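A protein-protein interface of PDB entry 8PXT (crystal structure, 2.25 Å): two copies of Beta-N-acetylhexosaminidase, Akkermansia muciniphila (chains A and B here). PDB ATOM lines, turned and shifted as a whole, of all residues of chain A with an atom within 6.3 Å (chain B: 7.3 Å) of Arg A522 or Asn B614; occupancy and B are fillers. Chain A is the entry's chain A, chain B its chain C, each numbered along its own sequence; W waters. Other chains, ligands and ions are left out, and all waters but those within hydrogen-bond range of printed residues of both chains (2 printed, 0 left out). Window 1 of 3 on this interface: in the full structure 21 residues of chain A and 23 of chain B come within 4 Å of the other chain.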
ATOM      1  N   TYR A 477       6.852  13.146 -22.221  1.00  0.00           N
ATOM      2  CA  TYR A 477       6.837  12.998 -23.671  1.00  0.00           C
ATOM      3  C   TYR A 477       6.538  14.323 -24.359  1.00  0.00           C
ATOM      4  O   TYR A 477       7.129  14.642 -25.397  1.00  0.00           O
ATOM      5  CB  TYR A 477       5.805  11.947 -24.087  1.00  0.00           C
ATOM      6  CG  TYR A 477       5.569  11.899 -25.582  1.00  0.00           C
ATOM      7  CD1 TYR A 477       6.412  11.176 -26.411  1.00  0.00           C
ATOM      8  CD2 TYR A 477       4.515  12.589 -26.162  1.00  0.00           C
ATOM      9  CE1 TYR A 477       6.209  11.135 -27.781  1.00  0.00           C
ATOM     10  CE2 TYR A 477       4.302  12.555 -27.534  1.00  0.00           C
ATOM     11  CZ  TYR A 477       5.156  11.825 -28.337  1.00  0.00           C
ATOM     12  OH  TYR A 477       4.958  11.778 -29.698  1.00  0.00           O
ATOM     13  N   PHE A 480       9.485  17.296 -23.119  1.00  0.00           N
ATOM     14  CA  PHE A 480      10.883  17.049 -23.428  1.00  0.00           C
ATOM     15  C   PHE A 480      10.993  16.243 -24.715  1.00  0.00           C
ATOM     16  O   PHE A 480      10.242  15.280 -24.900  1.00  0.00           O
ATOM     17  CB  PHE A 480      11.570  16.301 -22.272  1.00  0.00           C
ATOM     18  CG  PHE A 480      11.627  17.095 -21.001  1.00  0.00           C
ATOM     19  CD1 PHE A 480      12.607  18.055 -20.818  1.00  0.00           C
ATOM     20  CD2 PHE A 480      10.695  16.897 -19.999  1.00  0.00           C
ATOM     21  CE1 PHE A 480      12.659  18.796 -19.662  1.00  0.00           C
ATOM     22  CE2 PHE A 480      10.745  17.636 -18.834  1.00  0.00           C
ATOM     23  CZ  PHE A 480      11.727  18.589 -18.667  1.00  0.00           C
ATOM     24  N   PRO A 481      11.948  16.575 -25.604  1.00  0.00           N
ATOM     25  CA  PRO A 481      13.086  17.488 -25.426  1.00  0.00           C
ATOM     26  C   PRO A 481      12.901  18.966 -25.778  1.00  0.00           C
ATOM     27  O   PRO A 481      13.896  19.690 -25.736  1.00  0.00           O
ATOM     28  CB  PRO A 481      14.128  16.894 -26.379  1.00  0.00           C
ATOM     29  CG  PRO A 481      13.297  16.394 -27.513  1.00  0.00           C
ATOM     30  CD  PRO A 481      12.059  15.819 -26.866  1.00  0.00           C
ATOM     31  N   SER A 510      20.490  13.587 -23.336  1.00  0.00           N
ATOM     32  CA  SER A 510      19.423  12.601 -23.221  1.00  0.00           C
ATOM     33  C   SER A 510      19.850  11.389 -22.400  1.00  0.00           C
ATOM     34  O   SER A 510      18.983  10.681 -21.879  1.00  0.00           O
ATOM     35  CB  SER A 510      18.944  12.165 -24.610  1.00  0.00           C
ATOM     36  OG  SER A 510      19.898  11.350 -25.262  1.00  0.00           O
ATOM     37  N   ASP A 514      17.461   9.977 -19.284  1.00  0.00           N
ATOM     38  CA  ASP A 514      17.184   8.570 -19.011  1.00  0.00           C
ATOM     39  C   ASP A 514      17.481   8.237 -17.555  1.00  0.00           C
ATOM     40  O   ASP A 514      16.608   7.767 -16.818  1.00  0.00           O
ATOM     41  CB  ASP A 514      18.009   7.675 -19.938  1.00  0.00           C
ATOM     42  CG  ASP A 514      17.469   7.641 -21.352  1.00  0.00           C
ATOM     43  OD1 ASP A 514      16.254   7.873 -21.530  1.00  0.00           O
ATOM     44  OD2 ASP A 514      18.257   7.375 -22.286  1.00  0.00           O
ATOM     45  N   ILE A 518      13.238  10.576 -17.032  1.00  0.00           N
ATOM     46  CA  ILE A 518      12.425  11.462 -17.860  1.00  0.00           C
ATOM     47  C   ILE A 518      12.115  10.747 -19.173  1.00  0.00           C
ATOM     48  O   ILE A 518      13.017  10.481 -19.974  1.00  0.00           O
ATOM     49  CB  ILE A 518      13.134  12.798 -18.108  1.00  0.00           C
ATOM     50  CG1 ILE A 518      13.497  13.473 -16.781  1.00  0.00           C
ATOM     51  CG2 ILE A 518      12.266  13.723 -18.949  1.00  0.00           C
ATOM     52  CD1 ILE A 518      12.301  13.859 -15.931  1.00  0.00           C
ATOM     53  N   LYS A 519      10.832  10.452 -19.395  1.00  0.00           N
ATOM     54  CA  LYS A 519      10.381   9.737 -20.590  1.00  0.00           C
ATOM     55  C   LYS A 519      10.143  10.735 -21.724  1.00  0.00           C
ATOM     56  O   LYS A 519       9.020  10.987 -22.167  1.00  0.00           O
ATOM     57  CB  LYS A 519       9.126   8.927 -20.282  1.00  0.00           C
ATOM     58  CG  LYS A 519       9.328   7.826 -19.248  1.00  0.00           C
ATOM     59  CD  LYS A 519      10.439   6.877 -19.670  1.00  0.00           C
ATOM     60  CE  LYS A 519      10.398   5.563 -18.907  1.00  0.00           C
ATOM     61  NZ  LYS A 519      11.287   5.578 -17.712  1.00  0.00           N
ATOM     62  N   PHE A 520      11.249  11.298 -22.202  1.00  0.00           N
ATOM     63  CA  PHE A 520      11.200  12.254 -23.294  1.00  0.00           C
ATOM     64  C   PHE A 520      10.875  11.542 -24.606  1.00  0.00           C
ATOM     65  O   PHE A 520      11.039  10.326 -24.742  1.00  0.00           O
ATOM     66  CB  PHE A 520      12.532  12.994 -23.413  1.00  0.00           C
ATOM     67  CG  PHE A 520      13.694  12.092 -23.706  1.00  0.00           C
ATOM     68  CD1 PHE A 520      14.022  11.767 -25.010  1.00  0.00           C
ATOM     69  CD2 PHE A 520      14.447  11.555 -22.677  1.00  0.00           C
ATOM     70  CE1 PHE A 520      15.081  10.930 -25.281  1.00  0.00           C
ATOM     71  CE2 PHE A 520      15.508  10.715 -22.942  1.00  0.00           C
ATOM     72  CZ  PHE A 520      15.826  10.401 -24.243  1.00  0.00           C
ATOM     73  N   ALA A 521      10.410  12.324 -25.581  1.00  0.00           N
ATOM     74  CA  ALA A 521      10.049  11.772 -26.881  1.00  0.00           C
ATOM     75  C   ALA A 521      11.293  11.249 -27.593  1.00  0.00           C
ATOM     76  O   ALA A 521      12.315  11.938 -27.671  1.00  0.00           O
ATOM     77  CB  ALA A 521       9.351  12.830 -27.733  1.00  0.00           C
ATOM     78  N   ARG A 522      11.186  10.035 -28.136  1.00  0.00           N
ATOM     79  CA  ARG A 522      12.329   9.268 -28.618  1.00  0.00           C
ATOM     80  C   ARG A 522      12.727   9.602 -30.052  1.00  0.00           C
ATOM     81  O   ARG A 522      13.914   9.784 -30.342  1.00  0.00           O
ATOM     82  CB  ARG A 522      12.012   7.771 -28.508  1.00  0.00           C
ATOM     83  CG  ARG A 522      12.114   7.229 -27.097  1.00  0.00           C
ATOM     84  CD  ARG A 522      13.562   7.033 -26.707  1.00  0.00           C
ATOM     85  NE  ARG A 522      13.749   7.022 -25.262  1.00  0.00           N
ATOM     86  CZ  ARG A 522      14.917   6.839 -24.663  1.00  0.00           C
ATOM     87  NH1 ARG A 522      16.025   6.620 -25.355  1.00  0.00           N
ATOM     88  NH2 ARG A 522      14.978   6.878 -23.336  1.00  0.00           N
ATOM     89  N   ASN A 523      11.757   9.683 -30.959  1.00  0.00           N
ATOM     90  CA  ASN A 523      12.044   9.734 -32.388  1.00  0.00           C
ATOM     91  C   ASN A 523      12.357  11.144 -32.879  1.00  0.00           C
ATOM     92  O   ASN A 523      12.063  11.473 -34.032  1.00  0.00           O
ATOM     93  CB  ASN A 523      10.841   9.175 -33.158  1.00  0.00           C
ATOM     94  CG  ASN A 523      11.209   8.654 -34.532  1.00  0.00           C
ATOM     95  OD1 ASN A 523      12.356   8.280 -34.781  1.00  0.00           O
ATOM     96  ND2 ASN A 523      10.229   8.620 -35.432  1.00  0.00           N
ATOM     97  N   VAL A 524      12.973  11.977 -32.036  1.00  0.00           N
ATOM     98  CA  VAL A 524      13.022  13.420 -32.244  1.00  0.00           C
ATOM     99  C   VAL A 524      14.456  13.935 -32.314  1.00  0.00           C
ATOM    100  O   VAL A 524      14.812  14.691 -33.222  1.00  0.00           O
ATOM    101  CB  VAL A 524      12.235  14.168 -31.145  1.00  0.00           C
ATOM    102  CG1 VAL A 524      12.448  15.668 -31.267  1.00  0.00           C
ATOM    103  CG2 VAL A 524      10.758  13.816 -31.218  1.00  0.00           C
ATOM    104  N   ILE A 525      15.289  13.549 -31.349  1.00  0.00           N
ATOM    105  CA  ILE A 525      16.587  14.198 -31.177  1.00  0.00           C
ATOM    106  C   ILE A 525      17.453  14.043 -32.422  1.00  0.00           C
ATOM    107  O   ILE A 525      18.208  14.954 -32.784  1.00  0.00           O
ATOM    108  CB  ILE A 525      17.284  13.637 -29.924  1.00  0.00           C
ATOM    109  CG1 ILE A 525      16.587  14.172 -28.672  1.00  0.00           C
ATOM    110  CG2 ILE A 525      18.763  13.995 -29.925  1.00  0.00           C
ATOM    111  CD1 ILE A 525      16.829  13.343 -27.436  1.00  0.00           C
ATOM    112  N   SER A 526      17.354  12.903 -33.103  1.00  0.00           N
ATOM    113  CA  SER A 526      18.296  12.549 -34.156  1.00  0.00           C
ATOM    114  C   SER A 526      17.758  12.794 -35.561  1.00  0.00           C
ATOM    115  O   SER A 526      18.398  12.387 -36.536  1.00  0.00           O
ATOM    116  CB  SER A 526      18.709  11.085 -34.004  1.00  0.00           C
ATOM    117  OG  SER A 526      19.552  10.921 -32.876  1.00  0.00           O
ATOM    118  N   ALA B 562       1.768   1.237 -22.398  1.00  0.00           N
ATOM    119  CA  ALA B 562       2.895   1.837 -21.700  1.00  0.00           C
ATOM    120  C   ALA B 562       3.966   2.283 -22.683  1.00  0.00           C
ATOM    121  O   ALA B 562       4.052   1.801 -23.816  1.00  0.00           O
ATOM    122  CB  ALA B 562       3.510   0.867 -20.681  1.00  0.00           C
ATOM    123  N   SER B 563       4.779   3.231 -22.217  1.00  0.00           N
ATOM    124  CA  SER B 563       6.004   3.650 -22.880  1.00  0.00           C
ATOM    125  C   SER B 563       6.865   2.445 -23.235  1.00  0.00           C
ATOM    126  O   SER B 563       6.711   1.376 -22.636  1.00  0.00           O
ATOM    127  CB  SER B 563       6.774   4.601 -21.955  1.00  0.00           C
ATOM    128  OG  SER B 563       7.709   5.397 -22.662  1.00  0.00           O
ATOM    129  N   GLY B 564       7.761   2.595 -24.204  1.00  0.00           N
ATOM    130  CA  GLY B 564       8.842   1.648 -24.400  1.00  0.00           C
ATOM    131  C   GLY B 564       8.746   0.872 -25.703  1.00  0.00           C
ATOM    132  O   GLY B 564       7.964   1.183 -26.605  1.00  0.00           O
ATOM    133  N   LYS B 565       9.570  -0.170 -25.779  1.00  0.00           N
ATOM    134  CA  LYS B 565       9.808  -0.900 -27.016  1.00  0.00           C
ATOM    135  C   LYS B 565       8.796  -2.029 -27.175  1.00  0.00           C
ATOM    136  O   LYS B 565       8.763  -2.960 -26.364  1.00  0.00           O
ATOM    137  CB  LYS B 565      11.232  -1.457 -27.029  1.00  0.00           C
ATOM    138  CG  LYS B 565      12.314  -0.387 -27.099  1.00  0.00           C
ATOM    139  CD  LYS B 565      13.681  -0.938 -26.700  1.00  0.00           C
ATOM    140  CE  LYS B 565      14.740   0.157 -26.675  1.00  0.00           C
ATOM    141  NZ  LYS B 565      15.092   0.634 -28.043  1.00  0.00           N
ATOM    142  N   HIS B 566       7.978  -1.942 -28.220  1.00  0.00           N
ATOM    143  CA  HIS B 566       7.120  -3.034 -28.652  1.00  0.00           C
ATOM    144  C   HIS B 566       7.740  -3.691 -29.880  1.00  0.00           C
ATOM    145  O   HIS B 566       8.492  -3.061 -30.626  1.00  0.00           O
ATOM    146  CB  HIS B 566       5.709  -2.537 -28.977  1.00  0.00           C
ATOM    147  CG  HIS B 566       5.046  -1.815 -27.844  1.00  0.00           C
ATOM    148  ND1 HIS B 566       5.639  -0.756 -27.189  1.00  0.00           N
ATOM    149  CD2 HIS B 566       3.843  -1.998 -27.251  1.00  0.00           C
ATOM    150  CE1 HIS B 566       4.832  -0.322 -26.238  1.00  0.00           C
ATOM    151  NE2 HIS B 566       3.735  -1.058 -26.256  1.00  0.00           N
ATOM    152  N   LEU B 586       5.055   2.866 -36.248  1.00  0.00           N
ATOM    153  CA  LEU B 586       3.986   3.070 -35.286  1.00  0.00           C
ATOM    154  C   LEU B 586       3.418   4.466 -35.482  1.00  0.00           C
ATOM    155  O   LEU B 586       4.175   5.435 -35.621  1.00  0.00           O
ATOM    156  CB  LEU B 586       4.497   2.899 -33.856  1.00  0.00           C
ATOM    157  CG  LEU B 586       3.471   3.085 -32.740  1.00  0.00           C
ATOM    158  CD1 LEU B 586       2.409   2.001 -32.797  1.00  0.00           C
ATOM    159  CD2 LEU B 586       4.166   3.105 -31.388  1.00  0.00           C
ATOM    160  N   VAL B 593       5.396   8.107 -35.011  1.00  0.00           N
ATOM    161  CA  VAL B 593       6.182   8.331 -33.807  1.00  0.00           C
ATOM    162  C   VAL B 593       7.314   7.330 -33.654  1.00  0.00           C
ATOM    163  O   VAL B 593       8.090   7.436 -32.700  1.00  0.00           O
ATOM    164  CB  VAL B 593       5.291   8.323 -32.548  1.00  0.00           C
ATOM    165  CG1 VAL B 593       4.197   9.375 -32.674  1.00  0.00           C
ATOM    166  CG2 VAL B 593       4.691   6.946 -32.319  1.00  0.00           C
ATOM    167  N   SER B 594       7.436   6.366 -34.561  1.00  0.00           N
ATOM    168  CA  SER B 594       8.527   5.406 -34.506  1.00  0.00           C
ATOM    169  C   SER B 594       8.543   4.620 -35.806  1.00  0.00           C
ATOM    170  O   SER B 594       7.487   4.293 -36.350  1.00  0.00           O
ATOM    171  CB  SER B 594       8.382   4.454 -33.315  1.00  0.00           C
ATOM    172  OG  SER B 594       9.381   3.451 -33.354  1.00  0.00           O
ATOM    173  N   ARG B 595       9.745   4.319 -36.288  1.00  0.00           N
ATOM    174  CA  ARG B 595       9.909   3.658 -37.577  1.00  0.00           C
ATOM    175  C   ARG B 595      11.163   2.803 -37.527  1.00  0.00           C
ATOM    176  O   ARG B 595      12.256   3.316 -37.267  1.00  0.00           O
ATOM    177  CB  ARG B 595       9.998   4.685 -38.706  1.00  0.00           C
ATOM    178  CG  ARG B 595      10.081   4.085 -40.100  1.00  0.00           C
ATOM    179  CD  ARG B 595       9.650   5.097 -41.154  1.00  0.00           C
ATOM    180  NE  ARG B 595       9.537   4.499 -42.478  1.00  0.00           N
ATOM    181  CZ  ARG B 595      10.539   4.378 -43.339  1.00  0.00           C
ATOM    182  NH1 ARG B 595      11.752   4.828 -43.058  1.00  0.00           N
ATOM    183  NH2 ARG B 595      10.320   3.785 -44.509  1.00  0.00           N
ATOM    184  N   ASP B 596      10.998   1.504 -37.755  1.00  0.00           N
ATOM    185  CA  ASP B 596      12.108   0.564 -37.891  1.00  0.00           C
ATOM    186  C   ASP B 596      12.199   0.207 -39.369  1.00  0.00           C
ATOM    187  O   ASP B 596      11.379  -0.561 -39.882  1.00  0.00           O
ATOM    188  CB  ASP B 596      11.898  -0.671 -37.020  1.00  0.00           C
ATOM    189  CG  ASP B 596      13.038  -1.676 -37.135  1.00  0.00           C
ATOM    190  OD1 ASP B 596      13.949  -1.472 -37.966  1.00  0.00           O
ATOM    191  OD2 ASP B 596      13.017  -2.679 -36.390  1.00  0.00           O
ATOM    192  N   ILE B 612      11.185  -3.331 -34.189  1.00  0.00           N
ATOM    193  CA  ILE B 612      11.131  -2.754 -32.852  1.00  0.00           C
ATOM    194  C   ILE B 612      10.610  -1.329 -32.956  1.00  0.00           C
ATOM    195  O   ILE B 612      11.134  -0.524 -33.738  1.00  0.00           O
ATOM    196  CB  ILE B 612      12.513  -2.788 -32.180  1.00  0.00           C
ATOM    197  CG1 ILE B 612      13.084  -4.212 -32.184  1.00  0.00           C
ATOM    198  CG2 ILE B 612      12.424  -2.249 -30.762  1.00  0.00           C
ATOM    199  CD1 ILE B 612      12.221  -5.241 -31.477  1.00  0.00           C
ATOM    200  N   LEU B 613       9.587  -1.014 -32.164  1.00  0.00           N
ATOM    201  CA  LEU B 613       8.926   0.283 -32.194  1.00  0.00           C
ATOM    202  C   LEU B 613       8.934   0.906 -30.803  1.00  0.00           C
ATOM    203  O   LEU B 613       8.694   0.222 -29.805  1.00  0.00           O
ATOM    204  CB  LEU B 613       7.483   0.150 -32.700  1.00  0.00           C
ATOM    205  CG  LEU B 613       7.331  -0.448 -34.099  1.00  0.00           C
ATOM    206  CD1 LEU B 613       5.871  -0.652 -34.458  1.00  0.00           C
ATOM    207  CD2 LEU B 613       8.014   0.443 -35.122  1.00  0.00           C
ATOM    208  N   ASN B 614       9.205   2.207 -30.749  1.00  0.00           N
ATOM    209  CA  ASN B 614       9.233   2.957 -29.494  1.00  0.00           C
ATOM    210  C   ASN B 614       7.864   3.581 -29.270  1.00  0.00           C
ATOM    211  O   ASN B 614       7.512   4.580 -29.902  1.00  0.00           O
ATOM    212  CB  ASN B 614      10.309   4.037 -29.527  1.00  0.00           C
ATOM    213  CG  ASN B 614      11.709   3.473 -29.474  1.00  0.00           C
ATOM    214  OD1 ASN B 614      11.938   2.395 -28.920  1.00  0.00           O
ATOM    215  ND2 ASN B 614      12.661   4.203 -30.045  1.00  0.00           N
ATOM    216  N   ALA B 615       7.099   3.010 -28.368  1.00  0.00           N
ATOM    217  CA  ALA B 615       5.839   3.656 -28.046  1.00  0.00           C
ATOM    218  C   ALA B 615       6.076   4.773 -27.033  1.00  0.00           C
ATOM    219  O   ALA B 615       6.846   4.596 -26.087  1.00  0.00           O
ATOM    220  CB  ALA B 615       4.843   2.654 -27.474  1.00  0.00           C
ATOM    221  N   PRO B 616       5.453   5.933 -27.212  1.00  0.00           N
ATOM    222  CA  PRO B 616       5.409   6.910 -26.124  1.00  0.00           C
ATOM    223  C   PRO B 616       4.452   6.446 -25.041  1.00  0.00           C
ATOM    224  O   PRO B 616       3.684   5.496 -25.212  1.00  0.00           O
ATOM    225  CB  PRO B 616       4.905   8.183 -26.805  1.00  0.00           C
ATOM    226  CG  PRO B 616       4.120   7.697 -27.963  1.00  0.00           C
ATOM    227  CD  PRO B 616       4.832   6.463 -28.441  1.00  0.00           C
ATOM    228  N   ALA B 617       4.506   7.126 -23.906  1.00  0.00           N
ATOM    229  CA  ALA B 617       3.427   6.987 -22.946  1.00  0.00           C
ATOM    230  C   ALA B 617       2.112   7.211 -23.693  1.00  0.00           C
ATOM    231  O   ALA B 617       1.934   8.273 -24.307  1.00  0.00           O
ATOM    232  CB  ALA B 617       3.579   7.983 -21.802  1.00  0.00           C
HETATM  233  O   HOH W   1      12.017   5.409 -33.986  1.00  0.00           O
HETATM  234  O   HOH W   2       6.902   8.765 -22.992  1.00  0.00           O
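No position is printed for both chains.
The side-chain carboxylate (OD1) of Asp A514 lies within salt-bridge range of the guanidinium group (NH2) of Arg A522 (2.4 Å).
The backbone NH of Leu B586 sits at hydrogen-bond distance from the backbone carbonyl oxygen of Ser B594 (2.8 Å).
The backbone carbonyl oxygen (O) of Leu B586 lies within hydrogen-bond range of the backbone NH (N) of Val B593, at 3.0 Å.
The backbone NH (N) of Asn B614 is in hydrogen-bond range of the side-chain hydroxyl (OG) of Ser B594 (2.9 Å).
The backbone NH (N) of Tyr A477 lies within hydrogen-bond range of the backbone carbonyl oxygen (O) of Lys A519.
Of the printed residues of chain A, Pro B616 touches Tyr A477.
Of the printed residues of chain A, Ser B594 touches Asn A523.
Of the printed residues of chain A, Val B593 touches Tyr A477 and Asn A523.
Printed residues of chain B within 4 Å of Tyr A477: Val B593 (3.9 Å) and Pro B616 (3.4 Å).
Printed residues of chain B within 4 Å of Asn A523: Val B593 and Ser B594.
Phe A480 touches none of the printed residues of chain B.
The nearest printed residue of chain B that does not touch Asn A523 is Arg B595 (4.4 Å).
Water W1 lies within hydrogen-bond range of OD1 of Asn A523 (3.0 Å), OG of Ser B594 (3.3 Å) and N of Arg B595 (3.4 Å).
Water W2 lies within hydrogen-bond range of N of Ala B617 (3.0 Å), O of Lys A519 (3.2 Å) and OG of Ser B563 (3.5 Å).
Among the printed residues, pairs that only touch across the chains: Asn A523 with Val B593, Tyr A477 with Pro B616, Asn A523 with Ser B594, Tyr A477 with Val B593 and Arg A522 with Asn B614.
Of the 16 printed residues of chain B, 4 touch a printed residue of chain A.
Hydrophobic or aromatic side chains of chain B within 4 Å of the printed part of chain A: Val B593 and Pro B616.
Of the 14 printed residues of chain A, 3 touch a printed residue of chain B.
Hydrophobic or aromatic side chains of chain A within 4 Å of the printed part of chain B: Tyr A477.
Among the printed residues, no Asp or Glu carboxylate lies within 4 Å of a Lys or Arg side-chain nitrogen of the other chain.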
